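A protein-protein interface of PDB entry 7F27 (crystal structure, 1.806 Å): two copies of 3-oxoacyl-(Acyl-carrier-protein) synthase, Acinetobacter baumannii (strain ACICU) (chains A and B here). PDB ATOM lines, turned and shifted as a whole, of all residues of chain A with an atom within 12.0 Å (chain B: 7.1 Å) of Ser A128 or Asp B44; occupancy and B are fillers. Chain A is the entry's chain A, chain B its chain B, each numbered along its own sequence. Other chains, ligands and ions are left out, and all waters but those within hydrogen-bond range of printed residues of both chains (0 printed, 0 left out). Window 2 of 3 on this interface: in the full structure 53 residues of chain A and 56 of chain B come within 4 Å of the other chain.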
ATOM      1  N   ASP A 113       2.658   9.658  -8.150  1.00  0.00           N
ATOM      2  CA  ASP A 113       3.433   9.155  -7.015  1.00  0.00           C
ATOM      3  C   ASP A 113       2.876   9.686  -5.704  1.00  0.00           C
ATOM      4  O   ASP A 113       2.738   8.943  -4.723  1.00  0.00           O
ATOM      5  CB  ASP A 113       4.908   9.546  -7.137  1.00  0.00           C
ATOM      6  CG  ASP A 113       5.655   8.719  -8.163  1.00  0.00           C
ATOM      7  OD1 ASP A 113       5.051   7.773  -8.727  1.00  0.00           O
ATOM      8  OD2 ASP A 113       6.852   9.023  -8.404  1.00  0.00           O
ATOM      9  N   ALA A 114       2.563  10.983  -5.668  1.00  0.00           N
ATOM     10  CA  ALA A 114       1.983  11.565  -4.465  1.00  0.00           C
ATOM     11  C   ALA A 114       0.599  10.984  -4.178  1.00  0.00           C
ATOM     12  O   ALA A 114       0.253  10.753  -3.014  1.00  0.00           O
ATOM     13  CB  ALA A 114       1.928  13.084  -4.600  1.00  0.00           C
ATOM     14  N   VAL A 115      -0.202  10.726  -5.218  1.00  0.00           N
ATOM     15  CA  VAL A 115      -1.504  10.091  -4.995  1.00  0.00           C
ATOM     16  C   VAL A 115      -1.315   8.709  -4.375  1.00  0.00           C
ATOM     17  O   VAL A 115      -2.110   8.276  -3.530  1.00  0.00           O
ATOM     18  CB  VAL A 115      -2.310  10.025  -6.306  1.00  0.00           C
ATOM     19  CG1 VAL A 115      -3.517   9.103  -6.164  1.00  0.00           C
ATOM     20  CG2 VAL A 115      -2.767  11.417  -6.722  1.00  0.00           C
ATOM     21  N   GLY A 116      -0.245   8.010  -4.766  1.00  0.00           N
ATOM     22  CA  GLY A 116       0.042   6.714  -4.171  1.00  0.00           C
ATOM     23  C   GLY A 116       0.394   6.808  -2.698  1.00  0.00           C
ATOM     24  O   GLY A 116      -0.078   6.005  -1.889  1.00  0.00           O
ATOM     25  N   GLU A 117       1.222   7.790  -2.328  1.00  0.00           N
ATOM     26  CA  GLU A 117       1.538   8.014  -0.918  1.00  0.00           C
ATOM     27  C   GLU A 117       0.277   8.271  -0.104  1.00  0.00           C
ATOM     28  O   GLU A 117       0.099   7.708   0.982  1.00  0.00           O
ATOM     29  CB  GLU A 117       2.506   9.192  -0.774  1.00  0.00           C
ATOM     30  CG  GLU A 117       3.761   9.075  -1.602  1.00  0.00           C
ATOM     31  CD  GLU A 117       4.525  10.385  -1.710  1.00  0.00           C
ATOM     32  OE1 GLU A 117       4.184  11.364  -0.997  1.00  0.00           O
ATOM     33  OE2 GLU A 117       5.471  10.433  -2.516  1.00  0.00           O
ATOM     34  N   PHE A 118      -0.603   9.139  -0.615  1.00  0.00           N
ATOM     35  CA  PHE A 118      -1.850   9.468   0.069  1.00  0.00           C
ATOM     36  C   PHE A 118      -2.712   8.226   0.268  1.00  0.00           C
ATOM     37  O   PHE A 118      -3.350   8.060   1.316  1.00  0.00           O
ATOM     38  CB  PHE A 118      -2.586  10.539  -0.745  1.00  0.00           C
ATOM     39  CG  PHE A 118      -3.858  11.049  -0.118  1.00  0.00           C
ATOM     40  CD1 PHE A 118      -5.091  10.537  -0.506  1.00  0.00           C
ATOM     41  CD2 PHE A 118      -3.826  12.074   0.814  1.00  0.00           C
ATOM     42  CE1 PHE A 118      -6.267  11.014   0.044  1.00  0.00           C
ATOM     43  CE2 PHE A 118      -5.004  12.560   1.377  1.00  0.00           C
ATOM     44  CZ  PHE A 118      -6.227  12.031   0.988  1.00  0.00           C
ATOM     45  N   ALA A 119      -2.721   7.327  -0.715  1.00  0.00           N
ATOM     46  CA  ALA A 119      -3.510   6.107  -0.631  1.00  0.00           C
ATOM     47  C   ALA A 119      -2.837   5.000   0.171  1.00  0.00           C
ATOM     48  O   ALA A 119      -3.473   3.968   0.411  1.00  0.00           O
ATOM     49  CB  ALA A 119      -3.826   5.589  -2.033  1.00  0.00           C
ATOM     50  N   SER A 120      -1.575   5.173   0.577  1.00  0.00           N
ATOM     51  CA  SER A 120      -0.946   4.187   1.453  1.00  0.00           C
ATOM     52  C   SER A 120      -1.673   4.090   2.789  1.00  0.00           C
ATOM     53  O   SER A 120      -1.757   3.004   3.374  1.00  0.00           O
ATOM     54  CB  SER A 120       0.523   4.538   1.683  1.00  0.00           C
ATOM     55  OG  SER A 120       0.667   5.405   2.801  1.00  0.00           O
ATOM     56  N   MET A 121      -2.199   5.209   3.288  1.00  0.00           N
ATOM     57  CA  MET A 121      -3.007   5.170   4.500  1.00  0.00           C
ATOM     58  C   MET A 121      -4.366   4.537   4.236  1.00  0.00           C
ATOM     59  O   MET A 121      -4.867   3.757   5.053  1.00  0.00           O
ATOM     60  CB  MET A 121      -3.179   6.578   5.045  1.00  0.00           C
ATOM     61  CG  MET A 121      -3.916   6.627   6.354  1.00  0.00           C
ATOM     62  SD  MET A 121      -3.392   8.070   7.281  1.00  0.00           S
ATOM     63  CE  MET A 121      -1.813   8.364   6.504  1.00  0.00           C
ATOM     64  N   LEU A 122      -4.974   4.867   3.095  1.00  0.00           N
ATOM     65  CA  LEU A 122      -6.272   4.311   2.734  1.00  0.00           C
ATOM     66  C   LEU A 122      -6.227   2.793   2.635  1.00  0.00           C
ATOM     67  O   LEU A 122      -7.213   2.119   2.956  1.00  0.00           O
ATOM     68  CB  LEU A 122      -6.740   4.895   1.395  1.00  0.00           C
ATOM     69  CG  LEU A 122      -7.272   6.328   1.228  1.00  0.00           C
ATOM     70  CD1 LEU A 122      -6.486   7.334   2.031  1.00  0.00           C
ATOM     71  CD2 LEU A 122      -7.274   6.729  -0.252  1.00  0.00           C
ATOM     72  N   LEU A 123      -5.097   2.236   2.194  1.00  0.00           N
ATOM     73  CA  LEU A 123      -5.006   0.823   1.852  1.00  0.00           C
ATOM     74  C   LEU A 123      -4.226   0.017   2.885  1.00  0.00           C
ATOM     75  O   LEU A 123      -4.776  -0.917   3.475  1.00  0.00           O
ATOM     76  CB  LEU A 123      -4.386   0.674   0.450  1.00  0.00           C
ATOM     77  CG  LEU A 123      -5.086   1.456  -0.674  1.00  0.00           C
ATOM     78  CD1 LEU A 123      -4.311   1.390  -1.974  1.00  0.00           C
ATOM     79  CD2 LEU A 123      -6.518   0.973  -0.900  1.00  0.00           C
ATOM     80  N   HIS A 124      -2.963   0.356   3.138  1.00  0.00           N
ATOM     81  CA  HIS A 124      -2.115  -0.433   4.023  1.00  0.00           C
ATOM     82  C   HIS A 124      -1.985   0.153   5.423  1.00  0.00           C
ATOM     83  O   HIS A 124      -1.156  -0.333   6.201  1.00  0.00           O
ATOM     84  CB  HIS A 124      -0.716  -0.597   3.422  1.00  0.00           C
ATOM     85  CG  HIS A 124      -0.702  -1.252   2.078  1.00  0.00           C
ATOM     86  ND1 HIS A 124      -1.844  -1.719   1.460  1.00  0.00           N
ATOM     87  CD2 HIS A 124       0.320  -1.526   1.233  1.00  0.00           C
ATOM     88  CE1 HIS A 124      -1.526  -2.245   0.290  1.00  0.00           C
ATOM     89  NE2 HIS A 124      -0.220  -2.141   0.128  1.00  0.00           N
ATOM     90  N   GLN A 125      -2.749   1.200   5.754  1.00  0.00           N
ATOM     91  CA  GLN A 125      -2.708   1.860   7.062  1.00  0.00           C
ATOM     92  C   GLN A 125      -1.341   2.458   7.398  1.00  0.00           C
ATOM     93  O   GLN A 125      -1.234   3.298   8.300  1.00  0.00           O
ATOM     94  CB  GLN A 125      -3.133   0.885   8.169  1.00  0.00           C
ATOM     95  CG  GLN A 125      -4.625   0.894   8.490  1.00  0.00           C
ATOM     96  CD  GLN A 125      -5.480   0.178   7.447  1.00  0.00           C
ATOM     97  OE1 GLN A 125      -5.029  -0.105   6.331  1.00  0.00           O
ATOM     98  NE2 GLN A 125      -6.725  -0.119   7.812  1.00  0.00           N
ATOM     99  N   SER A 126      -0.297   2.041   6.681  1.00  0.00           N
ATOM    100  CA  SER A 126       1.064   2.487   6.956  1.00  0.00           C
ATOM    101  C   SER A 126       1.238   3.940   6.525  1.00  0.00           C
ATOM    102  O   SER A 126       1.093   4.270   5.342  1.00  0.00           O
ATOM    103  CB  SER A 126       2.062   1.580   6.235  1.00  0.00           C
ATOM    104  OG  SER A 126       3.400   1.961   6.503  1.00  0.00           O
ATOM    105  N   MET A 127       1.555   4.806   7.486  1.00  0.00           N
ATOM    106  CA  MET A 127       1.712   6.235   7.249  1.00  0.00           C
ATOM    107  C   MET A 127       3.150   6.633   6.912  1.00  0.00           C
ATOM    108  O   MET A 127       3.419   7.821   6.706  1.00  0.00           O
ATOM    109  CB  MET A 127       1.213   7.015   8.479  1.00  0.00           C
ATOM    110  CG  MET A 127       1.088   8.534   8.304  1.00  0.00           C
ATOM    111  SD  MET A 127       0.076   9.362   9.554  1.00  0.00           S
ATOM    112  CE  MET A 127       1.035  10.848   9.873  1.00  0.00           C
ATOM    113  N   SER A 128       4.079   5.675   6.815  1.00  0.00           N
ATOM    114  CA  SER A 128       5.461   6.032   6.499  1.00  0.00           C
ATOM    115  C   SER A 128       5.623   6.602   5.090  1.00  0.00           C
ATOM    116  O   SER A 128       6.764   6.867   4.687  1.00  0.00           O
ATOM    117  CB  SER A 128       6.391   4.820   6.682  1.00  0.00           C
ATOM    118  OG  SER A 128       6.276   3.877   5.624  1.00  0.00           O
ATOM    119  N   LYS A 129       4.531   6.801   4.341  1.00  0.00           N
ATOM    120  CA  LYS A 129       4.601   7.299   2.973  1.00  0.00           C
ATOM    121  C   LYS A 129       4.097   8.724   2.806  1.00  0.00           C
ATOM    122  O   LYS A 129       4.525   9.404   1.875  1.00  0.00           O
ATOM    123  CB  LYS A 129       3.821   6.381   2.024  1.00  0.00           C
ATOM    124  CG  LYS A 129       4.283   4.930   2.028  1.00  0.00           C
ATOM    125  CD  LYS A 129       5.803   4.804   2.006  1.00  0.00           C
ATOM    126  CE  LYS A 129       6.239   3.348   2.164  1.00  0.00           C
ATOM    127  NZ  LYS A 129       7.716   3.195   2.308  1.00  0.00           N
ATOM    128  N   ILE A 130       3.204   9.201   3.665  1.00  0.00           N
ATOM    129  CA  ILE A 130       2.800  10.603   3.619  1.00  0.00           C
ATOM    130  C   ILE A 130       3.912  11.449   4.227  1.00  0.00           C
ATOM    131  O   ILE A 130       4.492  11.092   5.260  1.00  0.00           O
ATOM    132  CB  ILE A 130       1.454  10.814   4.341  1.00  0.00           C
ATOM    133  CG1 ILE A 130       0.323  10.170   3.540  1.00  0.00           C
ATOM    134  CG2 ILE A 130       1.156  12.294   4.535  1.00  0.00           C
ATOM    135  CD1 ILE A 130      -1.074  10.634   3.953  1.00  0.00           C
ATOM    136  N   ASN A 131       4.244  12.557   3.566  1.00  0.00           N
ATOM    137  CA  ASN A 131       5.251  13.483   4.069  1.00  0.00           C
ATOM    138  C   ASN A 131       4.721  14.904   3.895  1.00  0.00           C
ATOM    139  O   ASN A 131       3.576  15.115   3.478  1.00  0.00           O
ATOM    140  CB  ASN A 131       6.598  13.252   3.373  1.00  0.00           C
ATOM    141  CG  ASN A 131       6.519  13.424   1.874  1.00  0.00           C
ATOM    142  OD1 ASN A 131       5.999  14.425   1.381  1.00  0.00           O
ATOM    143  ND2 ASN A 131       7.055  12.457   1.135  1.00  0.00           N
ATOM    144  N   ALA A 132       5.560  15.887   4.217  1.00  0.00           N
ATOM    145  CA  ALA A 132       5.134  17.281   4.248  1.00  0.00           C
ATOM    146  C   ALA A 132       4.856  17.860   2.867  1.00  0.00           C
ATOM    147  O   ALA A 132       4.287  18.955   2.783  1.00  0.00           O
ATOM    148  CB  ALA A 132       6.181  18.139   4.955  1.00  0.00           C
ATOM    149  N   THR A 133       5.220  17.166   1.787  1.00  0.00           N
ATOM    150  CA  THR A 133       4.906  17.640   0.443  1.00  0.00           C
ATOM    151  C   THR A 133       3.943  16.721  -0.296  1.00  0.00           C
ATOM    152  O   THR A 133       3.732  16.913  -1.501  1.00  0.00           O
ATOM    153  CB  THR A 133       6.180  17.831  -0.398  1.00  0.00           C
ATOM    154  OG1 THR A 133       6.869  16.581  -0.543  1.00  0.00           O
ATOM    155  CG2 THR A 133       7.105  18.868   0.236  1.00  0.00           C
ATOM    156  N   THR A 134       3.334  15.742   0.386  1.00  0.00           N
ATOM    157  CA  THR A 134       2.446  14.810  -0.308  1.00  0.00           C
ATOM    158  C   THR A 134       1.239  15.536  -0.897  1.00  0.00           C
ATOM    159  O   THR A 134       0.892  15.337  -2.068  1.00  0.00           O
ATOM    160  CB  THR A 134       1.995  13.689   0.638  1.00  0.00           C
ATOM    161  OG1 THR A 134       3.103  12.829   0.929  1.00  0.00           O
ATOM    162  CG2 THR A 134       0.889  12.862   0.000  1.00  0.00           C
ATOM    163  N   ARG A 137       2.165  17.928  -3.779  1.00  0.00           N
ATOM    164  CA  ARG A 137       2.491  17.252  -5.032  1.00  0.00           C
ATOM    165  C   ARG A 137       1.278  16.555  -5.646  1.00  0.00           C
ATOM    166  O   ARG A 137       1.178  16.459  -6.872  1.00  0.00           O
ATOM    167  CB  ARG A 137       3.637  16.254  -4.805  1.00  0.00           C
ATOM    168  CG  ARG A 137       5.024  16.897  -4.862  1.00  0.00           C
ATOM    169  CD  ARG A 137       6.151  15.901  -4.558  1.00  0.00           C
ATOM    170  NE  ARG A 137       6.096  15.457  -3.167  1.00  0.00           N
ATOM    171  CZ  ARG A 137       5.810  14.213  -2.784  1.00  0.00           C
ATOM    172  NH1 ARG A 137       5.567  13.265  -3.688  1.00  0.00           N
ATOM    173  NH2 ARG A 137       5.765  13.922  -1.489  1.00  0.00           N
ATOM    174  N   GLU B  40      -7.491   5.136  15.761  1.00  0.00           N
ATOM    175  CA  GLU B  40      -6.418   4.558  16.561  1.00  0.00           C
ATOM    176  C   GLU B  40      -5.569   3.600  15.739  1.00  0.00           C
ATOM    177  O   GLU B  40      -4.367   3.463  15.996  1.00  0.00           O
ATOM    178  CB  GLU B  40      -6.997   3.848  17.785  1.00  0.00           C
ATOM    179  CG  GLU B  40      -7.530   4.799  18.846  1.00  0.00           C
ATOM    180  CD  GLU B  40      -6.447   5.701  19.440  1.00  0.00           C
ATOM    181  OE1 GLU B  40      -5.247   5.365  19.316  1.00  0.00           O
ATOM    182  OE2 GLU B  40      -6.798   6.748  20.035  1.00  0.00           O
ATOM    183  N   GLN B  41      -6.174   2.954  14.738  1.00  0.00           N
ATOM    184  CA  GLN B  41      -5.470   2.020  13.870  1.00  0.00           C
ATOM    185  C   GLN B  41      -4.376   2.675  13.028  1.00  0.00           C
ATOM    186  O   GLN B  41      -3.634   1.959  12.347  1.00  0.00           O
ATOM    187  CB  GLN B  41      -6.482   1.333  12.961  1.00  0.00           C
ATOM    188  CG  GLN B  41      -7.457   2.310  12.350  1.00  0.00           C
ATOM    189  CD  GLN B  41      -8.194   1.736  11.160  1.00  0.00           C
ATOM    190  OE1 GLN B  41      -7.627   0.981  10.368  1.00  0.00           O
ATOM    191  NE2 GLN B  41      -9.463   2.106  11.016  1.00  0.00           N
ATOM    192  N   TYR B  42      -4.261   4.002  13.042  1.00  0.00           N
ATOM    193  CA  TYR B  42      -3.191   4.709  12.337  1.00  0.00           C
ATOM    194  C   TYR B  42      -2.186   5.158  13.393  1.00  0.00           C
ATOM    195  O   TYR B  42      -2.413   6.139  14.107  1.00  0.00           O
ATOM    196  CB  TYR B  42      -3.739   5.885  11.532  1.00  0.00           C
ATOM    197  CG  TYR B  42      -4.915   5.529  10.646  1.00  0.00           C
ATOM    198  CD1 TYR B  42      -4.728   4.847   9.448  1.00  0.00           C
ATOM    199  CD2 TYR B  42      -6.213   5.875  11.008  1.00  0.00           C
ATOM    200  CE1 TYR B  42      -5.803   4.519   8.634  1.00  0.00           C
ATOM    201  CE2 TYR B  42      -7.294   5.548  10.202  1.00  0.00           C
ATOM    202  CZ  TYR B  42      -7.084   4.872   9.017  1.00  0.00           C
ATOM    203  OH  TYR B  42      -8.154   4.544   8.211  1.00  0.00           O
ATOM    204  N   VAL B  43      -1.067   4.436  13.486  1.00  0.00           N
ATOM    205  CA  VAL B  43      -0.177   4.594  14.633  1.00  0.00           C
ATOM    206  C   VAL B  43       0.620   5.891  14.536  1.00  0.00           C
ATOM    207  O   VAL B  43       0.827   6.582  15.544  1.00  0.00           O
ATOM    208  CB  VAL B  43       0.741   3.363  14.766  1.00  0.00           C
ATOM    209  CG1 VAL B  43      -0.033   2.188  15.372  1.00  0.00           C
ATOM    210  CG2 VAL B  43       1.338   2.984  13.411  1.00  0.00           C
ATOM    211  N   ASP B  44       1.075   6.247  13.331  1.00  0.00           N
ATOM    212  CA  ASP B  44       1.870   7.461  13.162  1.00  0.00           C
ATOM    213  C   ASP B  44       1.036   8.731  13.283  1.00  0.00           C
ATOM    214  O   ASP B  44       1.603   9.815  13.462  1.00  0.00           O
ATOM    215  CB  ASP B  44       2.586   7.444  11.810  1.00  0.00           C
ATOM    216  CG  ASP B  44       3.610   6.327  11.704  1.00  0.00           C
ATOM    217  OD1 ASP B  44       4.424   6.180  12.641  1.00  0.00           O
ATOM    218  OD2 ASP B  44       3.611   5.607  10.678  1.00  0.00           O
ATOM    219  N   LEU B  45      -0.288   8.622  13.194  1.00  0.00           N
ATOM    220  CA  LEU B  45      -1.167   9.783  13.270  1.00  0.00           C
ATOM    221  C   LEU B  45      -1.322  10.210  14.724  1.00  0.00           C
ATOM    222  O   LEU B  45      -1.862   9.457  15.543  1.00  0.00           O
ATOM    223  CB  LEU B  45      -2.520   9.451  12.645  1.00  0.00           C
ATOM    224  CG  LEU B  45      -3.620  10.511  12.594  1.00  0.00           C
ATOM    225  CD1 LEU B  45      -3.219  11.675  11.713  1.00  0.00           C
ATOM    226  CD2 LEU B  45      -4.904   9.886  12.092  1.00  0.00           C
ATOM    227  N   ARG B  46      -0.851  11.413  15.049  1.00  0.00           N
ATOM    228  CA  ARG B  46      -0.905  11.869  16.434  1.00  0.00           C
ATOM    229  C   ARG B  46      -2.285  12.407  16.806  1.00  0.00           C
ATOM    230  O   ARG B  46      -2.768  12.161  17.918  1.00  0.00           O
ATOM    231  CB  ARG B  46       0.178  12.921  16.678  1.00  0.00           C
ATOM    232  CG  ARG B  46       1.603  12.345  16.653  1.00  0.00           C
ATOM    233  CD  ARG B  46       2.647  13.413  16.919  1.00  0.00           C
ATOM    234  NE  ARG B  46       2.303  14.648  16.223  1.00  0.00           N
ATOM    235  CZ  ARG B  46       2.589  14.903  14.948  1.00  0.00           C
ATOM    236  NH1 ARG B  46       3.247  14.015  14.209  1.00  0.00           N
ATOM    237  NH2 ARG B  46       2.214  16.062  14.414  1.00  0.00           N
ATOM    238  N   THR B  47      -2.942  13.127  15.898  1.00  0.00           N
ATOM    239  CA  THR B  47      -4.261  13.673  16.195  1.00  0.00           C
ATOM    240  C   THR B  47      -5.329  12.588  16.090  1.00  0.00           C
ATOM    241  O   THR B  47      -5.256  11.698  15.239  1.00  0.00           O
ATOM    242  CB  THR B  47      -4.586  14.838  15.255  1.00  0.00           C
ATOM    243  OG1 THR B  47      -5.744  15.537  15.729  1.00  0.00           O
ATOM    244  CG2 THR B  47      -4.839  14.356  13.824  1.00  0.00           C
ATOM    245  N   LYS B  48      -6.319  12.652  16.985  1.00  0.00           N
ATOM    246  CA  LYS B  48      -7.424  11.701  16.988  1.00  0.00           C
ATOM    247  C   LYS B  48      -8.753  12.429  17.143  1.00  0.00           C
ATOM    248  O   LYS B  48      -9.725  11.864  17.656  1.00  0.00           O
ATOM    249  CB  LYS B  48      -7.254  10.656  18.090  1.00  0.00           C
ATOM    250  CG  LYS B  48      -5.949   9.879  18.017  1.00  0.00           C
ATOM    251  CD  LYS B  48      -5.959   8.922  16.844  1.00  0.00           C
ATOM    252  CE  LYS B  48      -4.983   7.782  17.069  1.00  0.00           C
ATOM    253  NZ  LYS B  48      -3.625   8.078  16.560  1.00  0.00           N
ATOM    254  N   ASP B 203      -1.198  16.701   9.945  1.00  0.00           N
ATOM    255  CA  ASP B 203      -0.477  16.119  11.072  1.00  0.00           C
ATOM    256  C   ASP B 203       1.029  16.089  10.810  1.00  0.00           C
ATOM    257  O   ASP B 203       1.827  16.351  11.716  1.00  0.00           O
ATOM    258  CB  ASP B 203      -1.020  14.716  11.353  1.00  0.00           C
ATOM    259  CG  ASP B 203      -0.851  14.294  12.806  1.00  0.00           C
ATOM    260  OD1 ASP B 203       0.029  13.446  13.078  1.00  0.00           O
ATOM    261  OD2 ASP B 203      -1.602  14.807  13.671  1.00  0.00           O
ATOM    262  N   VAL B 204       1.442  15.789   9.573  1.00  0.00           N
ATOM    263  CA  VAL B 204       2.870  15.777   9.265  1.00  0.00           C
ATOM    264  C   VAL B 204       3.484  17.169   9.253  1.00  0.00           C
ATOM    265  O   VAL B 204       4.713  17.291   9.253  1.00  0.00           O
ATOM    266  CB  VAL B 204       3.151  15.081   7.918  1.00  0.00           C
ATOM    267  CG1 VAL B 204       2.805  13.596   8.011  1.00  0.00           C
ATOM    268  CG2 VAL B 204       2.378  15.757   6.802  1.00  0.00           C
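Printed residues of chain B that touch a printed residue of chain A: Gln B41, Tyr B42, Asp B44, Leu B45 and Val B204.
Of the 23 printed residues of chain A, 5 touch a printed residue of chain B.
Printed residues of chain A that touch a printed residue of chain B: Met A121, Gln A125, Met A127, Ser A128 and Asn A131.
Hydrophobic or aromatic side chains of chain A within 4 Å of the printed part of chain B: Met A121 and Met A127.
Among the printed residues, 8 pairs touch across the chains.
Among the printed residues, no Asp or Glu carboxylate lies within 4 Å of a Lys or Arg side-chain nitrogen of the other chain.
The side-chain amide nitrogen (NE2) of Gln A125 sits at hydrogen-bond distance from the side-chain amide oxygen (OE1) of Gln B41 (2.9 Å).
The backbone NH of Leu B45 is in hydrogen-bond range of the side-chain sulfur of Met A127 (3.7 Å).
The backbone carbonyl oxygen (O) of Ser A120 lies within hydrogen-bond range of the backbone NH (N) of Gln A125 (3.1 Å).
O of Leu A123 lies close to OE1 of Gln A125 (3.0 Å).
The backbone NH (N) of Thr A133 lies within hydrogen-bond range of the side-chain amide oxygen (OD1) of Asn A131 (2.9 Å).
The backbone NH (N) of Asn A131 is in hydrogen-bond range of the side-chain hydroxyl (OG1) of Thr A134 (2.9 Å).
The side-chain amide oxygen (OD1) of Asn A131 is in hydrogen-bond range of the guanidinium group (NH2) of Arg A137, at 2.9 Å.
The backbone carbonyl oxygen (O) of Tyr B42 sits at hydrogen-bond distance from the side-chain amino group (NZ) of Lys B48.
Of the printed residues of chain B, Met A121 touches Tyr B42.
Printed residues of chain B within 4 Å of Met A127: Asp B44 (3.5 Å), Leu B45 (3.7 Å) and Val B204 (3.8 Å).
Ser A128 touches just one residue of chain B: Asp B44 (3.9 Å).
Of the printed residues of chain A, Tyr B42 touches Met A121 and Gln A125.
No residue of chain A comes within 4 Å of Val B43.
Of chain A, only Met A127 (3.5 Å) and Ser A128 (3.9 Å) come within 4 Å of Asp B44.
Printed residues of chain A within 4 Å of Leu B45: Met A127.
No residue of chain A comes within 4 Å of Arg B46.
The nearest printed residue of chain B that does not touch Ser A128 is Val B43 (7.6 Å).
The nearest residue of chain A that does not touch Asp B44 is Ser A126 (5.1 Å).
The nearest printed residue of chain A that does not touch Tyr B42 is Met A127 (5.5 Å).
Met A121 touches Tyr B42 (CG to CE1, 3.6 Å).
CE1 of Tyr B42 touches CG of Gln A125, at 3.8 Å.
Met A127 touches Asp B44 (CB to OD2, 3.5 Å).
CE of Met A127 touches CG1 of Val B204, 3.8 Å away.
Asp B44 touches Ser A128.
Val B204 touches Asn A131.
No position is printed for both chains.
Of the 8 pairs that touch across the chains among the printed residues, none has its exchanged pair printed and touching as well.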
